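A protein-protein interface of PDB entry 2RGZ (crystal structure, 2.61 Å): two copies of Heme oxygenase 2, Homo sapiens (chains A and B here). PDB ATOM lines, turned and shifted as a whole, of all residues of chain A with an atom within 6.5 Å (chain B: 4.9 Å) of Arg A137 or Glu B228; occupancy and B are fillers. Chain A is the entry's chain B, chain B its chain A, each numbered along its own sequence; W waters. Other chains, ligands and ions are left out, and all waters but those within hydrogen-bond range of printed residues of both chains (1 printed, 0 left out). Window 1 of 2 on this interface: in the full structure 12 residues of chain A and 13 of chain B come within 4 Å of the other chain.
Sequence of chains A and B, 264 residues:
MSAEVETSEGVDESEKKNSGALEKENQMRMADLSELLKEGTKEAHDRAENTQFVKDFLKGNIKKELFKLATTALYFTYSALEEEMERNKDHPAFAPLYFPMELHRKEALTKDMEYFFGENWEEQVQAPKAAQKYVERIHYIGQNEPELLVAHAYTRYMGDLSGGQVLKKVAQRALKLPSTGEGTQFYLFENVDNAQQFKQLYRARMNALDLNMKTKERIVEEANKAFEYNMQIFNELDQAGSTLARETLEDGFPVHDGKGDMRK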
ATOM      1  N   GLN A 132     -37.427 -32.538  -4.286  1.00  0.00           N
ATOM      2  CA  GLN A 132     -36.217 -32.442  -3.482  1.00  0.00           C
ATOM      3  C   GLN A 132     -34.989 -32.603  -4.370  1.00  0.00           C
ATOM      4  O   GLN A 132     -33.923 -32.056  -4.082  1.00  0.00           O
ATOM      5  CB  GLN A 132     -36.198 -33.514  -2.400  1.00  0.00           C
ATOM      6  CG  GLN A 132     -35.022 -33.361  -1.453  1.00  0.00           C
ATOM      7  CD  GLN A 132     -34.852 -31.921  -0.991  1.00  0.00           C
ATOM      8  OE1 GLN A 132     -35.820 -31.159  -0.941  1.00  0.00           O
ATOM      9  NE2 GLN A 132     -33.624 -31.545  -0.640  1.00  0.00           N
ATOM     10  N   LYS A 133     -35.152 -33.372  -5.441  1.00  0.00           N
ATOM     11  CA  LYS A 133     -34.082 -33.588  -6.394  1.00  0.00           C
ATOM     12  C   LYS A 133     -33.819 -32.264  -7.104  1.00  0.00           C
ATOM     13  O   LYS A 133     -32.724 -31.700  -7.020  1.00  0.00           O
ATOM     14  CB  LYS A 133     -34.489 -34.637  -7.427  1.00  0.00           C
ATOM     15  CG  LYS A 133     -34.607 -36.042  -6.899  1.00  0.00           C
ATOM     16  CD  LYS A 133     -34.883 -37.016  -8.038  1.00  0.00           C
ATOM     17  CE  LYS A 133     -34.654 -38.457  -7.607  1.00  0.00           C
ATOM     18  NZ  LYS A 133     -34.830 -39.397  -8.736  1.00  0.00           N
ATOM     19  N   TYR A 134     -34.848 -31.780  -7.800  1.00  0.00           N
ATOM     20  CA  TYR A 134     -34.783 -30.519  -8.539  1.00  0.00           C
ATOM     21  C   TYR A 134     -34.261 -29.431  -7.617  1.00  0.00           C
ATOM     22  O   TYR A 134     -33.481 -28.576  -8.036  1.00  0.00           O
ATOM     23  CB  TYR A 134     -36.166 -30.151  -9.071  1.00  0.00           C
ATOM     24  CG  TYR A 134     -36.186 -28.940  -9.973  1.00  0.00           C
ATOM     25  CD1 TYR A 134     -35.042 -28.533 -10.650  1.00  0.00           C
ATOM     26  CD2 TYR A 134     -37.373 -28.238 -10.205  1.00  0.00           C
ATOM     27  CE1 TYR A 134     -35.072 -27.465 -11.541  1.00  0.00           C
ATOM     28  CE2 TYR A 134     -37.414 -27.163 -11.099  1.00  0.00           C
ATOM     29  CZ  TYR A 134     -36.257 -26.782 -11.766  1.00  0.00           C
ATOM     30  OH  TYR A 134     -36.272 -25.720 -12.664  1.00  0.00           O
ATOM     31  N   VAL A 135     -34.691 -29.476  -6.360  1.00  0.00           N
ATOM     32  CA  VAL A 135     -34.230 -28.517  -5.365  1.00  0.00           C
ATOM     33  C   VAL A 135     -32.732 -28.638  -5.092  1.00  0.00           C
ATOM     34  O   VAL A 135     -31.973 -27.741  -5.439  1.00  0.00           O
ATOM     35  CB  VAL A 135     -34.974 -28.690  -4.044  1.00  0.00           C
ATOM     36  CG1 VAL A 135     -34.207 -28.011  -2.912  1.00  0.00           C
ATOM     37  CG2 VAL A 135     -36.351 -28.089  -4.168  1.00  0.00           C
ATOM     38  N   GLU A 136     -32.302 -29.738  -4.471  1.00  0.00           N
ATOM     39  CA  GLU A 136     -30.879 -29.927  -4.163  1.00  0.00           C
ATOM     40  C   GLU A 136     -29.992 -29.417  -5.308  1.00  0.00           C
ATOM     41  O   GLU A 136     -28.932 -28.832  -5.075  1.00  0.00           O
ATOM     42  CB  GLU A 136     -30.589 -31.415  -3.856  1.00  0.00           C
ATOM     43  CG  GLU A 136     -30.991 -31.855  -2.427  1.00  0.00           C
ATOM     44  CD  GLU A 136     -31.018 -33.394  -2.205  1.00  0.00           C
ATOM     45  OE1 GLU A 136     -31.740 -34.093  -2.948  1.00  0.00           O
ATOM     46  OE2 GLU A 136     -30.341 -33.907  -1.267  1.00  0.00           O
ATOM     47  N   ARG A 137     -30.458 -29.614  -6.538  1.00  0.00           N
ATOM     48  CA  ARG A 137     -29.739 -29.200  -7.736  1.00  0.00           C
ATOM     49  C   ARG A 137     -29.609 -27.679  -7.853  1.00  0.00           C
ATOM     50  O   ARG A 137     -28.537 -27.151  -8.152  1.00  0.00           O
ATOM     51  CB  ARG A 137     -30.459 -29.742  -8.977  1.00  0.00           C
ATOM     52  CG  ARG A 137     -29.877 -29.269 -10.294  1.00  0.00           C
ATOM     53  CD  ARG A 137     -28.441 -29.746 -10.505  1.00  0.00           C
ATOM     54  NE  ARG A 137     -28.002 -29.560 -11.889  1.00  0.00           N
ATOM     55  CZ  ARG A 137     -26.874 -30.051 -12.394  1.00  0.00           C
ATOM     56  NH1 ARG A 137     -26.056 -30.766 -11.630  1.00  0.00           N
ATOM     57  NH2 ARG A 137     -26.561 -29.834 -13.667  1.00  0.00           N
ATOM     58  N   ILE A 138     -30.715 -26.989  -7.619  1.00  0.00           N
ATOM     59  CA  ILE A 138     -30.753 -25.547  -7.705  1.00  0.00           C
ATOM     60  C   ILE A 138     -29.779 -24.906  -6.728  1.00  0.00           C
ATOM     61  O   ILE A 138     -29.250 -23.828  -6.997  1.00  0.00           O
ATOM     62  CB  ILE A 138     -32.196 -25.048  -7.472  1.00  0.00           C
ATOM     63  CG1 ILE A 138     -33.094 -25.574  -8.598  1.00  0.00           C
ATOM     64  CG2 ILE A 138     -32.238 -23.541  -7.438  1.00  0.00           C
ATOM     65  CD1 ILE A 138     -34.574 -25.310  -8.396  1.00  0.00           C
ATOM     66  N   HIS A 139     -29.536 -25.560  -5.595  1.00  0.00           N
ATOM     67  CA  HIS A 139     -28.586 -25.025  -4.622  1.00  0.00           C
ATOM     68  C   HIS A 139     -27.154 -25.303  -5.101  1.00  0.00           C
ATOM     69  O   HIS A 139     -26.215 -24.560  -4.767  1.00  0.00           O
ATOM     70  CB  HIS A 139     -28.836 -25.625  -3.237  1.00  0.00           C
ATOM     71  CG  HIS A 139     -30.107 -25.145  -2.604  1.00  0.00           C
ATOM     72  ND1 HIS A 139     -30.365 -23.810  -2.380  1.00  0.00           N
ATOM     73  CD2 HIS A 139     -31.209 -25.817  -2.187  1.00  0.00           C
ATOM     74  CE1 HIS A 139     -31.572 -23.678  -1.858  1.00  0.00           C
ATOM     75  NE2 HIS A 139     -32.105 -24.881  -1.730  1.00  0.00           N
ATOM     76  N   TYR A 140     -26.985 -26.375  -5.874  1.00  0.00           N
ATOM     77  CA  TYR A 140     -25.677 -26.686  -6.431  1.00  0.00           C
ATOM     78  C   TYR A 140     -25.302 -25.554  -7.409  1.00  0.00           C
ATOM     79  O   TYR A 140     -24.339 -24.804  -7.185  1.00  0.00           O
ATOM     80  CB  TYR A 140     -25.688 -28.014  -7.212  1.00  0.00           C
ATOM     81  CG  TYR A 140     -24.435 -28.174  -8.050  1.00  0.00           C
ATOM     82  CD1 TYR A 140     -23.189 -28.334  -7.440  1.00  0.00           C
ATOM     83  CD2 TYR A 140     -24.474 -28.051  -9.445  1.00  0.00           C
ATOM     84  CE1 TYR A 140     -22.018 -28.356  -8.182  1.00  0.00           C
ATOM     85  CE2 TYR A 140     -23.292 -28.071 -10.207  1.00  0.00           C
ATOM     86  CZ  TYR A 140     -22.069 -28.220  -9.555  1.00  0.00           C
ATOM     87  OH  TYR A 140     -20.886 -28.201 -10.252  1.00  0.00           O
ATOM     88  N   ILE A 141     -26.081 -25.450  -8.491  1.00  0.00           N
ATOM     89  CA  ILE A 141     -25.862 -24.443  -9.523  1.00  0.00           C
ATOM     90  C   ILE A 141     -25.553 -23.040  -8.991  1.00  0.00           C
ATOM     91  O   ILE A 141     -24.504 -22.466  -9.302  1.00  0.00           O
ATOM     92  CB  ILE A 141     -27.067 -24.357 -10.461  1.00  0.00           C
ATOM     93  CG1 ILE A 141     -27.172 -25.655 -11.275  1.00  0.00           C
ATOM     94  CG2 ILE A 141     -26.955 -23.102 -11.350  1.00  0.00           C
ATOM     95  CD1 ILE A 141     -25.926 -26.009 -12.079  1.00  0.00           C
ATOM     96  N   GLY A 142     -26.465 -22.512  -8.182  1.00  0.00           N
ATOM     97  CA  GLY A 142     -26.283 -21.192  -7.624  1.00  0.00           C
ATOM     98  C   GLY A 142     -24.984 -21.059  -6.857  1.00  0.00           C
ATOM     99  O   GLY A 142     -24.360 -19.990  -6.847  1.00  0.00           O
ATOM    100  N   ASN A 144     -22.180 -23.321  -7.243  1.00  0.00           N
ATOM    101  CA  ASN A 144     -20.998 -23.729  -8.000  1.00  0.00           C
ATOM    102  C   ASN A 144     -20.919 -23.359  -9.486  1.00  0.00           C
ATOM    103  O   ASN A 144     -19.836 -23.053  -9.980  1.00  0.00           O
ATOM    104  CB  ASN A 144     -20.826 -25.231  -7.819  1.00  0.00           C
ATOM    105  CG  ASN A 144     -20.756 -25.610  -6.361  1.00  0.00           C
ATOM    106  OD1 ASN A 144     -19.760 -25.343  -5.698  1.00  0.00           O
ATOM    107  ND2 ASN A 144     -21.830 -26.203  -5.840  1.00  0.00           N
ATOM    108  N   GLU A 145     -22.046 -23.394 -10.198  1.00  0.00           N
ATOM    109  CA  GLU A 145     -22.058 -23.037 -11.615  1.00  0.00           C
ATOM    110  C   GLU A 145     -23.128 -21.974 -11.857  1.00  0.00           C
ATOM    111  O   GLU A 145     -24.123 -22.216 -12.536  1.00  0.00           O
ATOM    112  CB  GLU A 145     -22.322 -24.277 -12.482  1.00  0.00           C
ATOM    113  CG  GLU A 145     -21.161 -25.273 -12.514  1.00  0.00           C
ATOM    114  CD  GLU A 145     -21.446 -26.533 -13.331  1.00  0.00           C
ATOM    115  OE1 GLU A 145     -21.967 -26.425 -14.464  1.00  0.00           O
ATOM    116  OE2 GLU A 145     -21.131 -27.643 -12.841  1.00  0.00           O
ATOM    117  N   LEU A 148     -25.183 -20.814 -15.021  1.00  0.00           N
ATOM    118  CA  LEU A 148     -26.267 -21.666 -15.500  1.00  0.00           C
ATOM    119  C   LEU A 148     -27.574 -21.376 -14.776  1.00  0.00           C
ATOM    120  O   LEU A 148     -28.621 -21.904 -15.149  1.00  0.00           O
ATOM    121  CB  LEU A 148     -25.906 -23.144 -15.328  1.00  0.00           C
ATOM    122  CG  LEU A 148     -24.655 -23.643 -16.067  1.00  0.00           C
ATOM    123  CD1 LEU A 148     -24.419 -25.109 -15.734  1.00  0.00           C
ATOM    124  CD2 LEU A 148     -24.815 -23.451 -17.567  1.00  0.00           C
ATOM    125  N   HIS A 152     -32.424 -22.197 -15.201  1.00  0.00           N
ATOM    126  CA  HIS A 152     -33.527 -22.520 -14.310  1.00  0.00           C
ATOM    127  C   HIS A 152     -34.539 -21.376 -14.194  1.00  0.00           C
ATOM    128  O   HIS A 152     -35.740 -21.608 -14.044  1.00  0.00           O
ATOM    129  CB  HIS A 152     -32.986 -22.903 -12.930  1.00  0.00           C
ATOM    130  CG  HIS A 152     -32.266 -24.214 -12.920  1.00  0.00           C
ATOM    131  ND1 HIS A 152     -32.917 -25.417 -13.084  1.00  0.00           N
ATOM    132  CD2 HIS A 152     -30.942 -24.505 -12.881  1.00  0.00           C
ATOM    133  CE1 HIS A 152     -32.027 -26.389 -13.157  1.00  0.00           C
ATOM    134  NE2 HIS A 152     -30.820 -25.863 -13.038  1.00  0.00           N
ATOM    135  N   GLU A 222     -29.137 -27.786 -19.684  1.00  0.00           N
ATOM    136  CA  GLU A 222     -29.784 -27.787 -18.376  1.00  0.00           C
ATOM    137  C   GLU A 222     -31.244 -27.303 -18.401  1.00  0.00           C
ATOM    138  O   GLU A 222     -32.035 -27.681 -17.539  1.00  0.00           O
ATOM    139  CB  GLU A 222     -28.982 -26.929 -17.399  1.00  0.00           C
ATOM    140  CG  GLU A 222     -29.435 -27.083 -15.966  1.00  0.00           C
ATOM    141  CD  GLU A 222     -28.327 -27.585 -15.050  1.00  0.00           C
ATOM    142  OE1 GLU A 222     -27.480 -28.385 -15.516  1.00  0.00           O
ATOM    143  OE2 GLU A 222     -28.315 -27.189 -13.860  1.00  0.00           O
ATOM    144  N   LYS A 225     -32.632 -30.275 -18.937  1.00  0.00           N
ATOM    145  CA  LYS A 225     -32.457 -31.037 -17.717  1.00  0.00           C
ATOM    146  C   LYS A 225     -33.478 -30.541 -16.694  1.00  0.00           C
ATOM    147  O   LYS A 225     -34.053 -31.328 -15.940  1.00  0.00           O
ATOM    148  CB  LYS A 225     -31.043 -30.851 -17.171  1.00  0.00           C
ATOM    149  CG  LYS A 225     -30.744 -31.705 -15.957  1.00  0.00           C
ATOM    150  CD  LYS A 225     -29.275 -31.657 -15.584  1.00  0.00           C
ATOM    151  CE  LYS A 225     -28.992 -32.537 -14.379  1.00  0.00           C
ATOM    152  NZ  LYS A 225     -29.542 -33.905 -14.562  1.00  0.00           N
ATOM    153  N   TYR A 229     -36.788 -32.503 -14.867  1.00  0.00           N
ATOM    154  CA  TYR A 229     -36.990 -32.426 -13.437  1.00  0.00           C
ATOM    155  C   TYR A 229     -38.460 -32.174 -13.139  1.00  0.00           C
ATOM    156  O   TYR A 229     -39.013 -32.723 -12.188  1.00  0.00           O
ATOM    157  CB  TYR A 229     -36.131 -31.310 -12.854  1.00  0.00           C
ATOM    158  CG  TYR A 229     -34.789 -31.787 -12.371  1.00  0.00           C
ATOM    159  CD1 TYR A 229     -33.674 -30.945 -12.403  1.00  0.00           C
ATOM    160  CD2 TYR A 229     -34.638 -33.071 -11.833  1.00  0.00           C
ATOM    161  CE1 TYR A 229     -32.440 -31.371 -11.909  1.00  0.00           C
ATOM    162  CE2 TYR A 229     -33.415 -33.500 -11.337  1.00  0.00           C
ATOM    163  CZ  TYR A 229     -32.321 -32.645 -11.379  1.00  0.00           C
ATOM    164  OH  TYR A 229     -31.117 -33.068 -10.883  1.00  0.00           O
ATOM    165  N   ARG B  47     -25.917 -32.344   0.996  1.00  0.00           N
ATOM    166  CA  ARG B  47     -26.852 -32.792  -0.032  1.00  0.00           C
ATOM    167  C   ARG B  47     -26.700 -34.293  -0.294  1.00  0.00           C
ATOM    168  O   ARG B  47     -27.688 -34.992  -0.503  1.00  0.00           O
ATOM    169  CB  ARG B  47     -26.640 -32.011  -1.339  1.00  0.00           C
ATOM    170  CG  ARG B  47     -27.196 -30.592  -1.354  1.00  0.00           C
ATOM    171  CD  ARG B  47     -26.789 -29.869  -2.653  1.00  0.00           C
ATOM    172  NE  ARG B  47     -25.943 -28.703  -2.389  1.00  0.00           N
ATOM    173  CZ  ARG B  47     -24.829 -28.406  -3.054  1.00  0.00           C
ATOM    174  NH1 ARG B  47     -24.402 -29.182  -4.038  1.00  0.00           N
ATOM    175  NH2 ARG B  47     -24.124 -27.329  -2.726  1.00  0.00           N
ATOM    176  N   ASN B 224     -16.363 -29.908  -5.553  1.00  0.00           N
ATOM    177  CA  ASN B 224     -17.794 -29.633  -5.509  1.00  0.00           C
ATOM    178  C   ASN B 224     -18.482 -30.115  -6.779  1.00  0.00           C
ATOM    179  O   ASN B 224     -19.569 -30.697  -6.718  1.00  0.00           O
ATOM    180  CB  ASN B 224     -18.035 -28.136  -5.322  1.00  0.00           C
ATOM    181  CG  ASN B 224     -17.868 -27.701  -3.874  1.00  0.00           C
ATOM    182  OD1 ASN B 224     -18.710 -28.008  -3.025  1.00  0.00           O
ATOM    183  ND2 ASN B 224     -16.777 -27.001  -3.583  1.00  0.00           N
ATOM    184  N   LYS B 225     -17.863 -29.869  -7.927  1.00  0.00           N
ATOM    185  CA  LYS B 225     -18.428 -30.337  -9.188  1.00  0.00           C
ATOM    186  C   LYS B 225     -18.534 -31.861  -9.107  1.00  0.00           C
ATOM    187  O   LYS B 225     -19.554 -32.445  -9.463  1.00  0.00           O
ATOM    188  CB  LYS B 225     -17.516 -29.948 -10.365  1.00  0.00           C
ATOM    189  CG  LYS B 225     -18.028 -30.391 -11.735  1.00  0.00           C
ATOM    190  CD  LYS B 225     -17.166 -29.819 -12.857  1.00  0.00           C
ATOM    191  CE  LYS B 225     -17.778 -30.048 -14.235  1.00  0.00           C
ATOM    192  NZ  LYS B 225     -19.057 -29.300 -14.440  1.00  0.00           N
ATOM    193  N   ALA B 226     -17.462 -32.494  -8.637  1.00  0.00           N
ATOM    194  CA  ALA B 226     -17.397 -33.949  -8.482  1.00  0.00           C
ATOM    195  C   ALA B 226     -18.562 -34.498  -7.648  1.00  0.00           C
ATOM    196  O   ALA B 226     -19.176 -35.496  -8.029  1.00  0.00           O
ATOM    197  CB  ALA B 226     -16.074 -34.336  -7.851  1.00  0.00           C
ATOM    198  N   PHE B 227     -18.865 -33.862  -6.516  1.00  0.00           N
ATOM    199  CA  PHE B 227     -19.977 -34.326  -5.698  1.00  0.00           C
ATOM    200  C   PHE B 227     -21.244 -34.326  -6.566  1.00  0.00           C
ATOM    201  O   PHE B 227     -22.045 -35.264  -6.532  1.00  0.00           O
ATOM    202  CB  PHE B 227     -20.194 -33.408  -4.482  1.00  0.00           C
ATOM    203  CG  PHE B 227     -19.333 -33.744  -3.286  1.00  0.00           C
ATOM    204  CD1 PHE B 227     -18.026 -33.266  -3.184  1.00  0.00           C
ATOM    205  CD2 PHE B 227     -19.840 -34.536  -2.246  1.00  0.00           C
ATOM    206  CE1 PHE B 227     -17.241 -33.567  -2.067  1.00  0.00           C
ATOM    207  CE2 PHE B 227     -19.062 -34.839  -1.129  1.00  0.00           C
ATOM    208  CZ  PHE B 227     -17.768 -34.359  -1.036  1.00  0.00           C
ATOM    209  N   GLU B 228     -21.417 -33.277  -7.361  1.00  0.00           N
ATOM    210  CA  GLU B 228     -22.601 -33.181  -8.206  1.00  0.00           C
ATOM    211  C   GLU B 228     -22.634 -34.301  -9.247  1.00  0.00           C
ATOM    212  O   GLU B 228     -23.704 -34.738  -9.680  1.00  0.00           O
ATOM    213  CB  GLU B 228     -22.656 -31.814  -8.889  1.00  0.00           C
ATOM    214  CG  GLU B 228     -23.944 -31.551  -9.637  1.00  0.00           C
ATOM    215  CD  GLU B 228     -25.147 -31.580  -8.721  1.00  0.00           C
ATOM    216  OE1 GLU B 228     -25.001 -31.157  -7.550  1.00  0.00           O
ATOM    217  OE2 GLU B 228     -26.233 -32.006  -9.176  1.00  0.00           O
ATOM    218  N   TYR B 229     -21.462 -34.764  -9.660  1.00  0.00           N
ATOM    219  CA  TYR B 229     -21.422 -35.847 -10.620  1.00  0.00           C
ATOM    220  C   TYR B 229     -21.999 -37.072  -9.912  1.00  0.00           C
ATOM    221  O   TYR B 229     -22.732 -37.868 -10.515  1.00  0.00           O
ATOM    222  CB  TYR B 229     -19.982 -36.083 -11.098  1.00  0.00           C
ATOM    223  CG  TYR B 229     -19.589 -35.168 -12.242  1.00  0.00           C
ATOM    224  CD1 TYR B 229     -18.530 -34.270 -12.122  1.00  0.00           C
ATOM    225  CD2 TYR B 229     -20.310 -35.191 -13.450  1.00  0.00           C
ATOM    226  CE1 TYR B 229     -18.197 -33.408 -13.179  1.00  0.00           C
ATOM    227  CE2 TYR B 229     -19.991 -34.346 -14.504  1.00  0.00           C
ATOM    228  CZ  TYR B 229     -18.940 -33.451 -14.366  1.00  0.00           C
ATOM    229  OH  TYR B 229     -18.677 -32.569 -15.394  1.00  0.00           O
ATOM    230  N   ASN B 230     -21.679 -37.202  -8.622  1.00  0.00           N
ATOM    231  CA  ASN B 230     -22.194 -38.298  -7.807  1.00  0.00           C
ATOM    232  C   ASN B 230     -23.659 -38.028  -7.501  1.00  0.00           C
ATOM    233  O   ASN B 230     -24.474 -38.952  -7.430  1.00  0.00           O
ATOM    234  CB  ASN B 230     -21.404 -38.431  -6.504  1.00  0.00           C
ATOM    235  CG  ASN B 230     -20.039 -39.072  -6.715  1.00  0.00           C
ATOM    236  OD1 ASN B 230     -19.925 -40.292  -6.858  1.00  0.00           O
ATOM    237  ND2 ASN B 230     -18.996 -38.244  -6.753  1.00  0.00           N
ATOM    238  N   MET B 231     -23.998 -36.759  -7.323  1.00  0.00           N
ATOM    239  CA  MET B 231     -25.384 -36.418  -7.063  1.00  0.00           C
ATOM    240  C   MET B 231     -26.194 -36.868  -8.265  1.00  0.00           C
ATOM    241  O   MET B 231     -27.281 -37.413  -8.115  1.00  0.00           O
ATOM    242  CB  MET B 231     -25.558 -34.907  -6.866  1.00  0.00           C
ATOM    243  CG  MET B 231     -24.891 -34.361  -5.618  1.00  0.00           C
ATOM    244  SD  MET B 231     -25.382 -35.277  -4.124  1.00  0.00           S
ATOM    245  CE  MET B 231     -26.936 -34.473  -3.771  1.00  0.00           C
ATOM    246  N   GLN B 232     -25.661 -36.666  -9.465  1.00  0.00           N
ATOM    247  CA  GLN B 232     -26.421 -37.059 -10.640  1.00  0.00           C
ATOM    248  C   GLN B 232     -26.573 -38.559 -10.785  1.00  0.00           C
ATOM    249  O   GLN B 232     -27.577 -39.034 -11.308  1.00  0.00           O
ATOM    250  CB  GLN B 232     -25.820 -36.462 -11.916  1.00  0.00           C
ATOM    251  CG  GLN B 232     -26.070 -34.969 -12.061  1.00  0.00           C
ATOM    252  CD  GLN B 232     -27.540 -34.624 -11.967  1.00  0.00           C
ATOM    253  OE1 GLN B 232     -28.385 -35.321 -12.529  1.00  0.00           O
ATOM    254  NE2 GLN B 232     -27.858 -33.541 -11.261  1.00  0.00           N
HETATM  255  O   HOH W   1     -26.849 -31.031  -5.489  1.00  0.00           O
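The side-chain amide oxygen (OE1) of Gln B232 sits at hydrogen-bond distance from the side-chain amino group (NZ) of Lys A225, 2.7 Å away. The side-chain carboxylate of Glu A145 lies within salt-bridge range of the side-chain amino group of Lys B225 (3.1 Å). NE2 of Gln B232 lies close to NH1 of Arg A137 (3.3 Å). The side-chain carboxylate of Glu A136 lies close to the backbone carbonyl oxygen of Arg B47 (3.0 Å). The side-chain carboxylate of Glu B228 lies within salt-bridge range of the guanidinium group of Arg A137. The side-chain amide nitrogen of Gln B232 lies within hydrogen-bond range of the side-chain hydroxyl of Tyr A229 (3.3 Å).
The side-chain amide nitrogen of Gln B232 is in hydrogen-bond range of the side-chain carboxylate of Glu B228, 3.1 Å away. O of Tyr A140 sits close to ND2 of Asn A144, 3.2 Å away. The side-chain carboxylate (OE1) of Glu A222 lies within salt-bridge range of the guanidinium group (NH2) of Arg A137 (2.5 Å). The side-chain hydroxyl (OH) of Tyr A140 sits at hydrogen-bond distance from the side-chain carboxylate (OE2) of Glu A145 (2.7 Å). The side-chain amino group (NZ) of Lys B225 sits close to the side-chain hydroxyl (OH) of Tyr B229.
Tyr A140 touches Arg B47. CE1 of Tyr A140 touches O of Asn B224 (3.7 Å). CA of Lys B225 touches OH of Tyr A140, 3.4 Å away. Glu B228 touches Tyr A140. Asn A144 touches Asn B224 (OD1 to CB, 3.3 Å).
Of chain B, only Glu B228 (2.8 Å) and Gln B232 (3.3 Å) come within 4 Å of Arg A137. Of the printed residues of chain B, Glu A145 touches Lys B225 (3.1 Å). Printed residues of chain B within 4 Å of Asn A144: Asn B224. Printed residues of chain A within 4 Å of Gln B232: Arg A137, Lys A225 and Tyr A229. Printed residues of chain A within 4 Å of Lys B225: Tyr A140 (3.4 Å) and Glu A145 (3.1 Å). Lys A133 touches none of the printed residues of chain B. The nearest residue of chain A that does not touch Glu B228 is Glu A136 (5.2 Å). The nearest printed residue of chain A that does not touch Asn B224 is Glu A145 (7.0 Å).
Of the 10 printed residues of chain B, 5 touch a printed residue of chain A. Printed residues of chain B that touch a printed residue of chain A: Arg B47, Asn B224, Lys B225, Glu B228 and Gln B232. Along chain B the printed residues that touch a printed residue of chain A span positions 47 to 232. Of the 18 printed residues of chain A, 7 touch a printed residue of chain B. Hydrophobic or aromatic side chains of chain A that line the printed part of chain B: Tyr A140 and Tyr A229. Along chain A the printed residues that touch a printed residue of chain B span positions 136 to 229. Among the printed residues, 11 pairs touch across the chains. Among the printed residues, Asp or Glu carboxylates within 4 Å of a Lys or Arg side-chain nitrogen of the other chain: Arg A137 with Glu B228 (2.8 Å) and Glu A145 with Lys B225 (3.1 Å).
Positions printed for both chains: 225 and 229.
Water W1 lies within hydrogen-bond range of the side-chain carboxylate of Glu B228, the backbone carbonyl oxygen of Glu A136 and the guanidinium group of Arg B47.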
